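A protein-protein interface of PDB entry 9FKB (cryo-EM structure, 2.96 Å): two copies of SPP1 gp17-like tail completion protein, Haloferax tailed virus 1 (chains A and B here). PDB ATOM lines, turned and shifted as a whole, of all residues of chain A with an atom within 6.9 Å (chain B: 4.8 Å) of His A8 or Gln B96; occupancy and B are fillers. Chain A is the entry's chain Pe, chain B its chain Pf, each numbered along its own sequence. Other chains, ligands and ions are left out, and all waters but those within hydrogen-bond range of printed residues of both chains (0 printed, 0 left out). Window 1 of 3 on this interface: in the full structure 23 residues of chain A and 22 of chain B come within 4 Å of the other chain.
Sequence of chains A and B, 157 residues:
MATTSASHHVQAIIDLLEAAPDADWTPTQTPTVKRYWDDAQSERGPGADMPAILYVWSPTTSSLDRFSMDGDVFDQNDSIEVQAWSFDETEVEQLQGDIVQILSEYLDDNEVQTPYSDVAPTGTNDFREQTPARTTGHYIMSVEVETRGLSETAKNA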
ATOM      1  N   SER A   5     -38.072   4.575  -0.314  1.00  0.00           N
ATOM      2  CA  SER A   5     -37.427   5.812   0.129  1.00  0.00           C
ATOM      3  C   SER A   5     -35.921   5.843  -0.208  1.00  0.00           C
ATOM      4  O   SER A   5     -35.125   6.509   0.458  1.00  0.00           O
ATOM      5  CB  SER A   5     -37.717   6.066   1.610  1.00  0.00           C
ATOM      6  OG  SER A   5     -37.287   7.356   2.019  1.00  0.00           O
ATOM      7  N   ALA A   6     -35.535   5.168  -1.300  1.00  0.00           N
ATOM      8  CA  ALA A   6     -34.143   4.992  -1.700  1.00  0.00           C
ATOM      9  C   ALA A   6     -33.563   6.264  -2.335  1.00  0.00           C
ATOM     10  O   ALA A   6     -34.252   7.042  -2.995  1.00  0.00           O
ATOM     11  CB  ALA A   6     -34.038   3.810  -2.622  1.00  0.00           C
ATOM     12  N   SER A   7     -32.246   6.448  -2.182  1.00  0.00           N
ATOM     13  CA  SER A   7     -31.532   7.639  -2.645  1.00  0.00           C
ATOM     14  C   SER A   7     -31.290   7.600  -4.161  1.00  0.00           C
ATOM     15  O   SER A   7     -31.186   8.639  -4.817  1.00  0.00           O
ATOM     16  CB  SER A   7     -30.251   7.810  -1.835  1.00  0.00           C
ATOM     17  OG  SER A   7     -29.157   8.366  -2.565  1.00  0.00           O
ATOM     18  N   HIS A   8     -31.227   6.389  -4.734  1.00  0.00           N
ATOM     19  CA  HIS A   8     -30.851   6.180  -6.130  1.00  0.00           C
ATOM     20  C   HIS A   8     -31.568   4.962  -6.703  1.00  0.00           C
ATOM     21  O   HIS A   8     -31.967   4.067  -5.972  1.00  0.00           O
ATOM     22  CB  HIS A   8     -29.355   5.945  -6.163  1.00  0.00           C
ATOM     23  CG  HIS A   8     -28.744   5.718  -7.502  1.00  0.00           C
ATOM     24  ND1 HIS A   8     -28.700   4.473  -8.151  1.00  0.00           N
ATOM     25  CD2 HIS A   8     -28.060   6.592  -8.266  1.00  0.00           C
ATOM     26  CE1 HIS A   8     -28.033   4.646  -9.287  1.00  0.00           C
ATOM     27  NE2 HIS A   8     -27.633   5.920  -9.373  1.00  0.00           N
ATOM     28  N   HIS A   9     -31.751   4.939  -8.024  1.00  0.00           N
ATOM     29  CA  HIS A   9     -32.598   3.961  -8.689  1.00  0.00           C
ATOM     30  C   HIS A   9     -32.146   2.519  -8.484  1.00  0.00           C
ATOM     31  O   HIS A   9     -32.994   1.650  -8.298  1.00  0.00           O
ATOM     32  CB  HIS A   9     -32.766   4.300 -10.169  1.00  0.00           C
ATOM     33  CG  HIS A   9     -31.552   4.703 -10.931  1.00  0.00           C
ATOM     34  ND1 HIS A   9     -30.955   5.955 -10.850  1.00  0.00           N
ATOM     35  CD2 HIS A   9     -30.900   4.043 -11.894  1.00  0.00           C
ATOM     36  CE1 HIS A   9     -29.979   6.026 -11.742  1.00  0.00           C
ATOM     37  NE2 HIS A   9     -29.922   4.862 -12.382  1.00  0.00           N
ATOM     38  N   VAL A  10     -30.836   2.257  -8.484  1.00  0.00           N
ATOM     39  CA  VAL A  10     -30.318   0.904  -8.303  1.00  0.00           C
ATOM     40  C   VAL A  10     -30.759   0.337  -6.955  1.00  0.00           C
ATOM     41  O   VAL A  10     -31.242  -0.789  -6.879  1.00  0.00           O
ATOM     42  CB  VAL A  10     -28.793   0.830  -8.515  1.00  0.00           C
ATOM     43  CG1 VAL A  10     -28.235  -0.521  -8.087  1.00  0.00           C
ATOM     44  CG2 VAL A  10     -28.454   1.020  -9.978  1.00  0.00           C
ATOM     45  N   GLN A  11     -30.631   1.132  -5.891  1.00  0.00           N
ATOM     46  CA  GLN A  11     -31.099   0.714  -4.585  1.00  0.00           C
ATOM     47  C   GLN A  11     -32.621   0.609  -4.536  1.00  0.00           C
ATOM     48  O   GLN A  11     -33.153  -0.297  -3.904  1.00  0.00           O
ATOM     49  CB  GLN A  11     -30.553   1.628  -3.487  1.00  0.00           C
ATOM     50  CG  GLN A  11     -30.802   1.059  -2.095  1.00  0.00           C
ATOM     51  CD  GLN A  11     -30.146  -0.290  -1.883  1.00  0.00           C
ATOM     52  OE1 GLN A  11     -28.945  -0.445  -2.088  1.00  0.00           O
ATOM     53  NE2 GLN A  11     -30.908  -1.279  -1.439  1.00  0.00           N
ATOM     54  N   ALA A  12     -33.337   1.508  -5.216  1.00  0.00           N
ATOM     55  CA  ALA A  12     -34.796   1.479  -5.262  1.00  0.00           C
ATOM     56  C   ALA A  12     -35.305   0.144  -5.816  1.00  0.00           C
ATOM     57  O   ALA A  12     -36.141  -0.502  -5.197  1.00  0.00           O
ATOM     58  CB  ALA A  12     -35.325   2.652  -6.056  1.00  0.00           C
ATOM     59  N   ILE A  13     -34.767  -0.301  -6.953  1.00  0.00           N
ATOM     60  CA  ILE A  13     -35.202  -1.547  -7.556  1.00  0.00           C
ATOM     61  C   ILE A  13     -34.819  -2.770  -6.725  1.00  0.00           C
ATOM     62  O   ILE A  13     -35.609  -3.709  -6.623  1.00  0.00           O
ATOM     63  CB  ILE A  13     -34.740  -1.614  -9.023  1.00  0.00           C
ATOM     64  CG1 ILE A  13     -35.523  -0.560  -9.810  1.00  0.00           C
ATOM     65  CG2 ILE A  13     -34.907  -3.019  -9.606  1.00  0.00           C
ATOM     66  CD1 ILE A  13     -35.826  -0.898 -11.259  1.00  0.00           C
ATOM     67  N   TRP A  37     -21.971  -5.451  -8.787  1.00  0.00           N
ATOM     68  CA  TRP A  37     -20.631  -5.340  -8.228  1.00  0.00           C
ATOM     69  C   TRP A  37     -20.430  -5.985  -6.843  1.00  0.00           C
ATOM     70  O   TRP A  37     -19.339  -5.874  -6.276  1.00  0.00           O
ATOM     71  CB  TRP A  37     -20.253  -3.858  -8.233  1.00  0.00           C
ATOM     72  CG  TRP A  37     -21.046  -2.985  -7.304  1.00  0.00           C
ATOM     73  CD1 TRP A  37     -20.775  -2.780  -5.986  1.00  0.00           C
ATOM     74  CD2 TRP A  37     -22.199  -2.152  -7.604  1.00  0.00           C
ATOM     75  NE1 TRP A  37     -21.661  -1.881  -5.455  1.00  0.00           N
ATOM     76  CE2 TRP A  37     -22.557  -1.473  -6.413  1.00  0.00           C
ATOM     77  CE3 TRP A  37     -22.975  -1.910  -8.749  1.00  0.00           C
ATOM     78  CZ2 TRP A  37     -23.639  -0.575  -6.346  1.00  0.00           C
ATOM     79  CZ3 TRP A  37     -24.040  -1.028  -8.692  1.00  0.00           C
ATOM     80  CH2 TRP A  37     -24.367  -0.374  -7.500  1.00  0.00           C
ATOM     81  N   SER A  58     -27.276  -0.027 -13.214  1.00  0.00           N
ATOM     82  CA  SER A  58     -27.739   0.941 -14.201  1.00  0.00           C
ATOM     83  C   SER A  58     -26.854   0.911 -15.450  1.00  0.00           C
ATOM     84  O   SER A  58     -25.718   1.379 -15.393  1.00  0.00           O
ATOM     85  CB  SER A  58     -27.791   2.310 -13.588  1.00  0.00           C
ATOM     86  OG  SER A  58     -28.397   3.227 -14.478  1.00  0.00           O
ATOM     87  N   SER A  62     -28.553   8.004 -17.436  1.00  0.00           N
ATOM     88  CA  SER A  62     -29.796   8.642 -17.014  1.00  0.00           C
ATOM     89  C   SER A  62     -29.901  10.048 -17.608  1.00  0.00           C
ATOM     90  O   SER A  62     -28.915  10.779 -17.607  1.00  0.00           O
ATOM     91  CB  SER A  62     -29.883   8.732 -15.524  1.00  0.00           C
ATOM     92  OG  SER A  62     -30.123   7.468 -14.943  1.00  0.00           O
ATOM     93  N   ASP A  78     -34.431   7.156 -15.948  1.00  0.00           N
ATOM     94  CA  ASP A  78     -33.419   6.265 -15.404  1.00  0.00           C
ATOM     95  C   ASP A  78     -33.614   4.849 -15.941  1.00  0.00           C
ATOM     96  O   ASP A  78     -34.745   4.395 -16.101  1.00  0.00           O
ATOM     97  CB  ASP A  78     -33.521   6.246 -13.877  1.00  0.00           C
ATOM     98  CG  ASP A  78     -33.241   7.605 -13.244  1.00  0.00           C
ATOM     99  OD1 ASP A  78     -32.186   8.177 -13.561  1.00  0.00           O
ATOM    100  OD2 ASP A  78     -34.067   8.085 -12.417  1.00  0.00           O
ATOM    101  N   ILE A  80     -32.293   0.573 -15.775  1.00  0.00           N
ATOM    102  CA  ILE A  80     -31.766  -0.531 -14.984  1.00  0.00           C
ATOM    103  C   ILE A  80     -31.844  -1.829 -15.779  1.00  0.00           C
ATOM    104  O   ILE A  80     -32.811  -2.063 -16.494  1.00  0.00           O
ATOM    105  CB  ILE A  80     -32.514  -0.616 -13.641  1.00  0.00           C
ATOM    106  CG1 ILE A  80     -32.013   0.547 -12.785  1.00  0.00           C
ATOM    107  CG2 ILE A  80     -32.325  -1.977 -12.965  1.00  0.00           C
ATOM    108  CD1 ILE A  80     -32.594   0.662 -11.394  1.00  0.00           C
ATOM    109  N   PRO A 115     -40.272   6.328  -4.916  1.00  0.00           N
ATOM    110  CA  PRO A 115     -40.077   7.766  -5.092  1.00  0.00           C
ATOM    111  C   PRO A 115     -40.223   8.232  -6.546  1.00  0.00           C
ATOM    112  O   PRO A 115     -39.690   9.283  -6.907  1.00  0.00           O
ATOM    113  CB  PRO A 115     -38.612   7.951  -4.626  1.00  0.00           C
ATOM    114  CG  PRO A 115     -37.940   6.691  -5.113  1.00  0.00           C
ATOM    115  CD  PRO A 115     -38.994   5.615  -4.915  1.00  0.00           C
ATOM    116  N   TYR A 116     -40.952   7.475  -7.392  1.00  0.00           N
ATOM    117  CA  TYR A 116     -41.032   7.724  -8.833  1.00  0.00           C
ATOM    118  C   TYR A 116     -42.477   7.820  -9.321  1.00  0.00           C
ATOM    119  O   TYR A 116     -43.394   7.343  -8.670  1.00  0.00           O
ATOM    120  CB  TYR A 116     -40.299   6.618  -9.588  1.00  0.00           C
ATOM    121  CG  TYR A 116     -38.849   6.489  -9.197  1.00  0.00           C
ATOM    122  CD1 TYR A 116     -37.998   7.589  -9.291  1.00  0.00           C
ATOM    123  CD2 TYR A 116     -38.325   5.285  -8.735  1.00  0.00           C
ATOM    124  CE1 TYR A 116     -36.663   7.515  -8.916  1.00  0.00           C
ATOM    125  CE2 TYR A 116     -36.989   5.201  -8.357  1.00  0.00           C
ATOM    126  CZ  TYR A 116     -36.163   6.317  -8.437  1.00  0.00           C
ATOM    127  OH  TYR A 116     -34.861   6.241  -8.035  1.00  0.00           O
ATOM    128  N   VAL B  92     -19.869   7.793  -3.589  1.00  0.00           N
ATOM    129  CA  VAL B  92     -19.970   8.209  -4.986  1.00  0.00           C
ATOM    130  C   VAL B  92     -21.410   8.573  -5.357  1.00  0.00           C
ATOM    131  O   VAL B  92     -21.642   9.515  -6.117  1.00  0.00           O
ATOM    132  CB  VAL B  92     -19.376   7.188  -5.979  1.00  0.00           C
ATOM    133  CG1 VAL B  92     -17.861   7.172  -5.922  1.00  0.00           C
ATOM    134  CG2 VAL B  92     -19.910   5.786  -5.770  1.00  0.00           C
ATOM    135  N   GLU B  93     -22.387   7.861  -4.788  1.00  0.00           N
ATOM    136  CA  GLU B  93     -23.805   8.107  -5.019  1.00  0.00           C
ATOM    137  C   GLU B  93     -24.238   9.427  -4.382  1.00  0.00           C
ATOM    138  O   GLU B  93     -24.936  10.220  -5.013  1.00  0.00           O
ATOM    139  CB  GLU B  93     -24.582   6.907  -4.499  1.00  0.00           C
ATOM    140  CG  GLU B  93     -26.083   6.976  -4.655  1.00  0.00           C
ATOM    141  CD  GLU B  93     -26.769   5.805  -3.969  1.00  0.00           C
ATOM    142  OE1 GLU B  93     -26.536   4.641  -4.397  1.00  0.00           O
ATOM    143  OE2 GLU B  93     -27.537   6.043  -3.008  1.00  0.00           O
ATOM    144  N   GLN B  94     -23.791   9.689  -3.149  1.00  0.00           N
ATOM    145  CA  GLN B  94     -24.024  10.961  -2.485  1.00  0.00           C
ATOM    146  C   GLN B  94     -23.364  12.114  -3.240  1.00  0.00           C
ATOM    147  O   GLN B  94     -23.984  13.149  -3.421  1.00  0.00           O
ATOM    148  CB  GLN B  94     -23.554  10.882  -1.041  1.00  0.00           C
ATOM    149  CG  GLN B  94     -24.475  10.019  -0.190  1.00  0.00           C
ATOM    150  CD  GLN B  94     -23.996   9.780   1.225  1.00  0.00           C
ATOM    151  OE1 GLN B  94     -22.863  10.099   1.597  1.00  0.00           O
ATOM    152  NE2 GLN B  94     -24.874   9.211   2.040  1.00  0.00           N
ATOM    153  N   LEU B  95     -22.141  11.927  -3.740  1.00  0.00           N
ATOM    154  CA  LEU B  95     -21.468  12.933  -4.548  1.00  0.00           C
ATOM    155  C   LEU B  95     -22.222  13.199  -5.844  1.00  0.00           C
ATOM    156  O   LEU B  95     -22.359  14.355  -6.220  1.00  0.00           O
ATOM    157  CB  LEU B  95     -20.023  12.515  -4.832  1.00  0.00           C
ATOM    158  CG  LEU B  95     -18.997  13.191  -3.930  1.00  0.00           C
ATOM    159  CD1 LEU B  95     -19.336  13.043  -2.458  1.00  0.00           C
ATOM    160  CD2 LEU B  95     -17.621  12.613  -4.187  1.00  0.00           C
ATOM    161  N   GLN B  96     -22.727  12.172  -6.532  1.00  0.00           N
ATOM    162  CA  GLN B  96     -23.546  12.396  -7.716  1.00  0.00           C
ATOM    163  C   GLN B  96     -24.762  13.262  -7.372  1.00  0.00           C
ATOM    164  O   GLN B  96     -25.011  14.270  -8.037  1.00  0.00           O
ATOM    165  CB  GLN B  96     -23.920  11.067  -8.361  1.00  0.00           C
ATOM    166  CG  GLN B  96     -24.870  11.226  -9.532  1.00  0.00           C
ATOM    167  CD  GLN B  96     -25.054   9.935 -10.297  1.00  0.00           C
ATOM    168  OE1 GLN B  96     -26.007   9.183 -10.070  1.00  0.00           O
ATOM    169  NE2 GLN B  96     -24.139   9.658 -11.213  1.00  0.00           N
ATOM    170  N   GLY B  97     -25.504  12.885  -6.322  1.00  0.00           N
ATOM    171  CA  GLY B  97     -26.636  13.655  -5.815  1.00  0.00           C
ATOM    172  C   GLY B  97     -26.248  15.100  -5.502  1.00  0.00           C
ATOM    173  O   GLY B  97     -26.912  16.035  -5.937  1.00  0.00           O
ATOM    174  N   ASP B  98     -25.133  15.290  -4.798  1.00  0.00           N
ATOM    175  CA  ASP B  98     -24.610  16.602  -4.454  1.00  0.00           C
ATOM    176  C   ASP B  98     -24.260  17.432  -5.693  1.00  0.00           C
ATOM    177  O   ASP B  98     -24.663  18.582  -5.776  1.00  0.00           O
ATOM    178  CB  ASP B  98     -23.411  16.476  -3.511  1.00  0.00           C
ATOM    179  CG  ASP B  98     -23.728  15.969  -2.107  1.00  0.00           C
ATOM    180  OD1 ASP B  98     -24.897  16.064  -1.664  1.00  0.00           O
ATOM    181  OD2 ASP B  98     -22.782  15.554  -1.406  1.00  0.00           O
ATOM    182  N   ILE B  99     -23.540  16.869  -6.670  1.00  0.00           N
ATOM    183  CA  ILE B  99     -23.102  17.601  -7.857  1.00  0.00           C
ATOM    184  C   ILE B  99     -24.307  18.080  -8.666  1.00  0.00           C
ATOM    185  O   ILE B  99     -24.341  19.226  -9.110  1.00  0.00           O
ATOM    186  CB  ILE B  99     -22.150  16.756  -8.729  1.00  0.00           C
ATOM    187  CG1 ILE B  99     -20.829  16.462  -8.013  1.00  0.00           C
ATOM    188  CG2 ILE B  99     -21.878  17.430 -10.078  1.00  0.00           C
ATOM    189  CD1 ILE B  99     -20.148  15.195  -8.494  1.00  0.00           C
ATOM    190  N   VAL B 100     -25.313  17.214  -8.842  1.00  0.00           N
ATOM    191  CA  VAL B 100     -26.560  17.595  -9.496  1.00  0.00           C
ATOM    192  C   VAL B 100     -27.224  18.740  -8.732  1.00  0.00           C
ATOM    193  O   VAL B 100     -27.655  19.695  -9.358  1.00  0.00           O
ATOM    194  CB  VAL B 100     -27.500  16.387  -9.672  1.00  0.00           C
ATOM    195  CG1 VAL B 100     -28.898  16.770 -10.130  1.00  0.00           C
ATOM    196  CG2 VAL B 100     -26.908  15.391 -10.646  1.00  0.00           C
ATOM    197  N   THR B 124     -26.636  11.576 -16.086  1.00  0.00           N
ATOM    198  CA  THR B 124     -25.774  11.010 -15.059  1.00  0.00           C
ATOM    199  C   THR B 124     -25.457   9.555 -15.395  1.00  0.00           C
ATOM    200  O   THR B 124     -26.301   8.838 -15.941  1.00  0.00           O
ATOM    201  CB  THR B 124     -26.403  11.115 -13.662  1.00  0.00           C
ATOM    202  OG1 THR B 124     -27.654  10.423 -13.612  1.00  0.00           O
ATOM    203  CG2 THR B 124     -26.624  12.536 -13.187  1.00  0.00           C
ATOM    204  N   ASN B 125     -24.238   9.118 -15.038  1.00  0.00           N
ATOM    205  CA  ASN B 125     -23.824   7.735 -15.216  1.00  0.00           C
ATOM    206  C   ASN B 125     -23.462   7.097 -13.877  1.00  0.00           C
ATOM    207  O   ASN B 125     -22.903   7.736 -12.980  1.00  0.00           O
ATOM    208  CB  ASN B 125     -22.634   7.645 -16.162  1.00  0.00           C
ATOM    209  CG  ASN B 125     -22.900   8.288 -17.503  1.00  0.00           C
ATOM    210  OD1 ASN B 125     -23.652   7.750 -18.304  1.00  0.00           O
ATOM    211  ND2 ASN B 125     -22.288   9.437 -17.753  1.00  0.00           N
ATOM    212  N   ASP B 126     -23.757   5.800 -13.790  1.00  0.00           N
ATOM    213  CA  ASP B 126     -23.219   4.943 -12.750  1.00  0.00           C
ATOM    214  C   ASP B 126     -22.218   3.996 -13.411  1.00  0.00           C
ATOM    215  O   ASP B 126     -22.536   3.424 -14.449  1.00  0.00           O
ATOM    216  CB  ASP B 126     -24.381   4.224 -12.058  1.00  0.00           C
ATOM    217  CG  ASP B 126     -23.993   3.403 -10.841  1.00  0.00           C
ATOM    218  OD1 ASP B 126     -22.796   3.301 -10.553  1.00  0.00           O
ATOM    219  OD2 ASP B 126     -24.900   2.908 -10.145  1.00  0.00           O
ATOM    220  N   ARG B 128     -20.402   1.858 -11.049  1.00  0.00           N
ATOM    221  CA  ARG B 128     -20.105   0.980  -9.923  1.00  0.00           C
ATOM    222  C   ARG B 128     -20.068  -0.491 -10.331  1.00  0.00           C
ATOM    223  O   ARG B 128     -19.345  -1.258  -9.713  1.00  0.00           O
ATOM    224  CB  ARG B 128     -21.096   1.196  -8.786  1.00  0.00           C
ATOM    225  CG  ARG B 128     -20.920   2.546  -8.115  1.00  0.00           C
ATOM    226  CD  ARG B 128     -21.952   2.780  -7.024  1.00  0.00           C
ATOM    227  NE  ARG B 128     -23.300   2.874  -7.555  1.00  0.00           N
ATOM    228  CZ  ARG B 128     -24.410   3.121  -6.860  1.00  0.00           C
ATOM    229  NH1 ARG B 128     -25.561   3.157  -7.500  1.00  0.00           N
ATOM    230  NH2 ARG B 128     -24.400   3.323  -5.548  1.00  0.00           N
ATOM    231  N   MET B 141     -18.768   7.276 -10.368  1.00  0.00           N
ATOM    232  CA  MET B 141     -20.046   7.739 -10.897  1.00  0.00           C
ATOM    233  C   MET B 141     -19.810   9.113 -11.528  1.00  0.00           C
ATOM    234  O   MET B 141     -18.818   9.762 -11.214  1.00  0.00           O
ATOM    235  CB  MET B 141     -21.122   7.812  -9.802  1.00  0.00           C
ATOM    236  CG  MET B 141     -21.481   6.451  -9.208  1.00  0.00           C
ATOM    237  SD  MET B 141     -22.758   6.441  -7.912  1.00  0.00           S
ATOM    238  CE  MET B 141     -24.255   6.563  -8.894  1.00  0.00           C
ATOM    239  N   SER B 142     -20.690   9.570 -12.432  1.00  0.00           N
ATOM    240  CA  SER B 142     -20.457  10.845 -13.104  1.00  0.00           C
ATOM    241  C   SER B 142     -21.732  11.652 -13.376  1.00  0.00           C
ATOM    242  O   SER B 142     -22.845  11.118 -13.405  1.00  0.00           O
ATOM    243  CB  SER B 142     -19.634  10.660 -14.360  1.00  0.00           C
ATOM    244  OG  SER B 142     -20.418  10.202 -15.448  1.00  0.00           O
ATOM    245  N   VAL B 143     -21.536  12.964 -13.570  1.00  0.00           N
ATOM    246  CA  VAL B 143     -22.554  13.890 -14.041  1.00  0.00           C
ATOM    247  C   VAL B 143     -22.123  14.456 -15.392  1.00  0.00           C
ATOM    248  O   VAL B 143     -21.007  14.939 -15.545  1.00  0.00           O
ATOM    249  CB  VAL B 143     -22.810  15.012 -13.018  1.00  0.00           C
ATOM    250  CG1 VAL B 143     -23.888  15.974 -13.495  1.00  0.00           C
ATOM    251  CG2 VAL B 143     -23.204  14.435 -11.668  1.00  0.00           C
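No position is printed for both chains.
Of the 9 pairs that touch across the chains among the printed residues, none has its exchanged pair printed and touching as well.
Hydrophobic or aromatic side chains of chain A within 4 Å of the printed part of chain B: His A8 and Trp A37.
Along chain A the printed residues that touch a printed residue of chain B span positions 7 to 62.
Among the printed residues, no Asp or Glu carboxylate lies within 4 Å of a Lys or Arg side-chain nitrogen of the other chain.
The side-chain hydroxyl of Ser A7 lies within hydrogen-bond range of the side-chain carboxylate of Glu B93, 2.9 Å away.
The guanidinium group (NH1) of Arg B128 lies close to a ring nitrogen (ND1) of His A8 (3.5 Å).
The backbone NH (N) of Ser A62 sits at hydrogen-bond distance from the backbone carbonyl oxygen (O) of Thr B124.
His A8 touches just these residues of chain B: Glu B93, Gln B96, Asp B126, Arg B128 and Met B141.
Gln B96 touches just one residue of chain A: His A8 (3.7 Å).
Of the printed residues of chain B, Trp A37 touches Arg B128.
Printed residues of chain A within 4 Å of Glu B93: Ser A7 and His A8.
Val A10 touches none of the printed residues of chain B.
Val B92 touches none of the printed residues of chain A.
The nearest printed residue of chain B that does not touch His A8 is Thr B124 (6.2 Å).
The nearest printed residue of chain A that does not touch Thr B124 is Asp A78 (5.1 Å).
Among the printed residues, pairs that only touch across the chains: His A8 with Glu B93, His A8 with Gln B96, His A8 with Asp B126, His A8 with Met B141, Trp A37 with Arg B128 and Ser A58 with Asp B126.
The side-chain amide nitrogen of Gln B96 sits at hydrogen-bond distance from the backbone carbonyl oxygen of Ser B142 (2.9 Å).
The backbone NH (N) of Glu B93 lies within hydrogen-bond range of the side-chain sulfur (SD) of Met B141.
A ring nitrogen (NE2) of His A9 sits at hydrogen-bond distance from the side-chain hydroxyl (OG) of Ser A58, 3.1 Å away.
NH2 of Arg B128 is in salt-bridge range of OE1 of Glu B93, 2.8 Å away.
The guanidinium group (NE) of Arg B128 is in hydrogen-bond range of the side-chain sulfur (SD) of Met B141.
NE2 of Gln B96 sits at hydrogen-bond distance from O of Asn B125 (2.9 Å).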
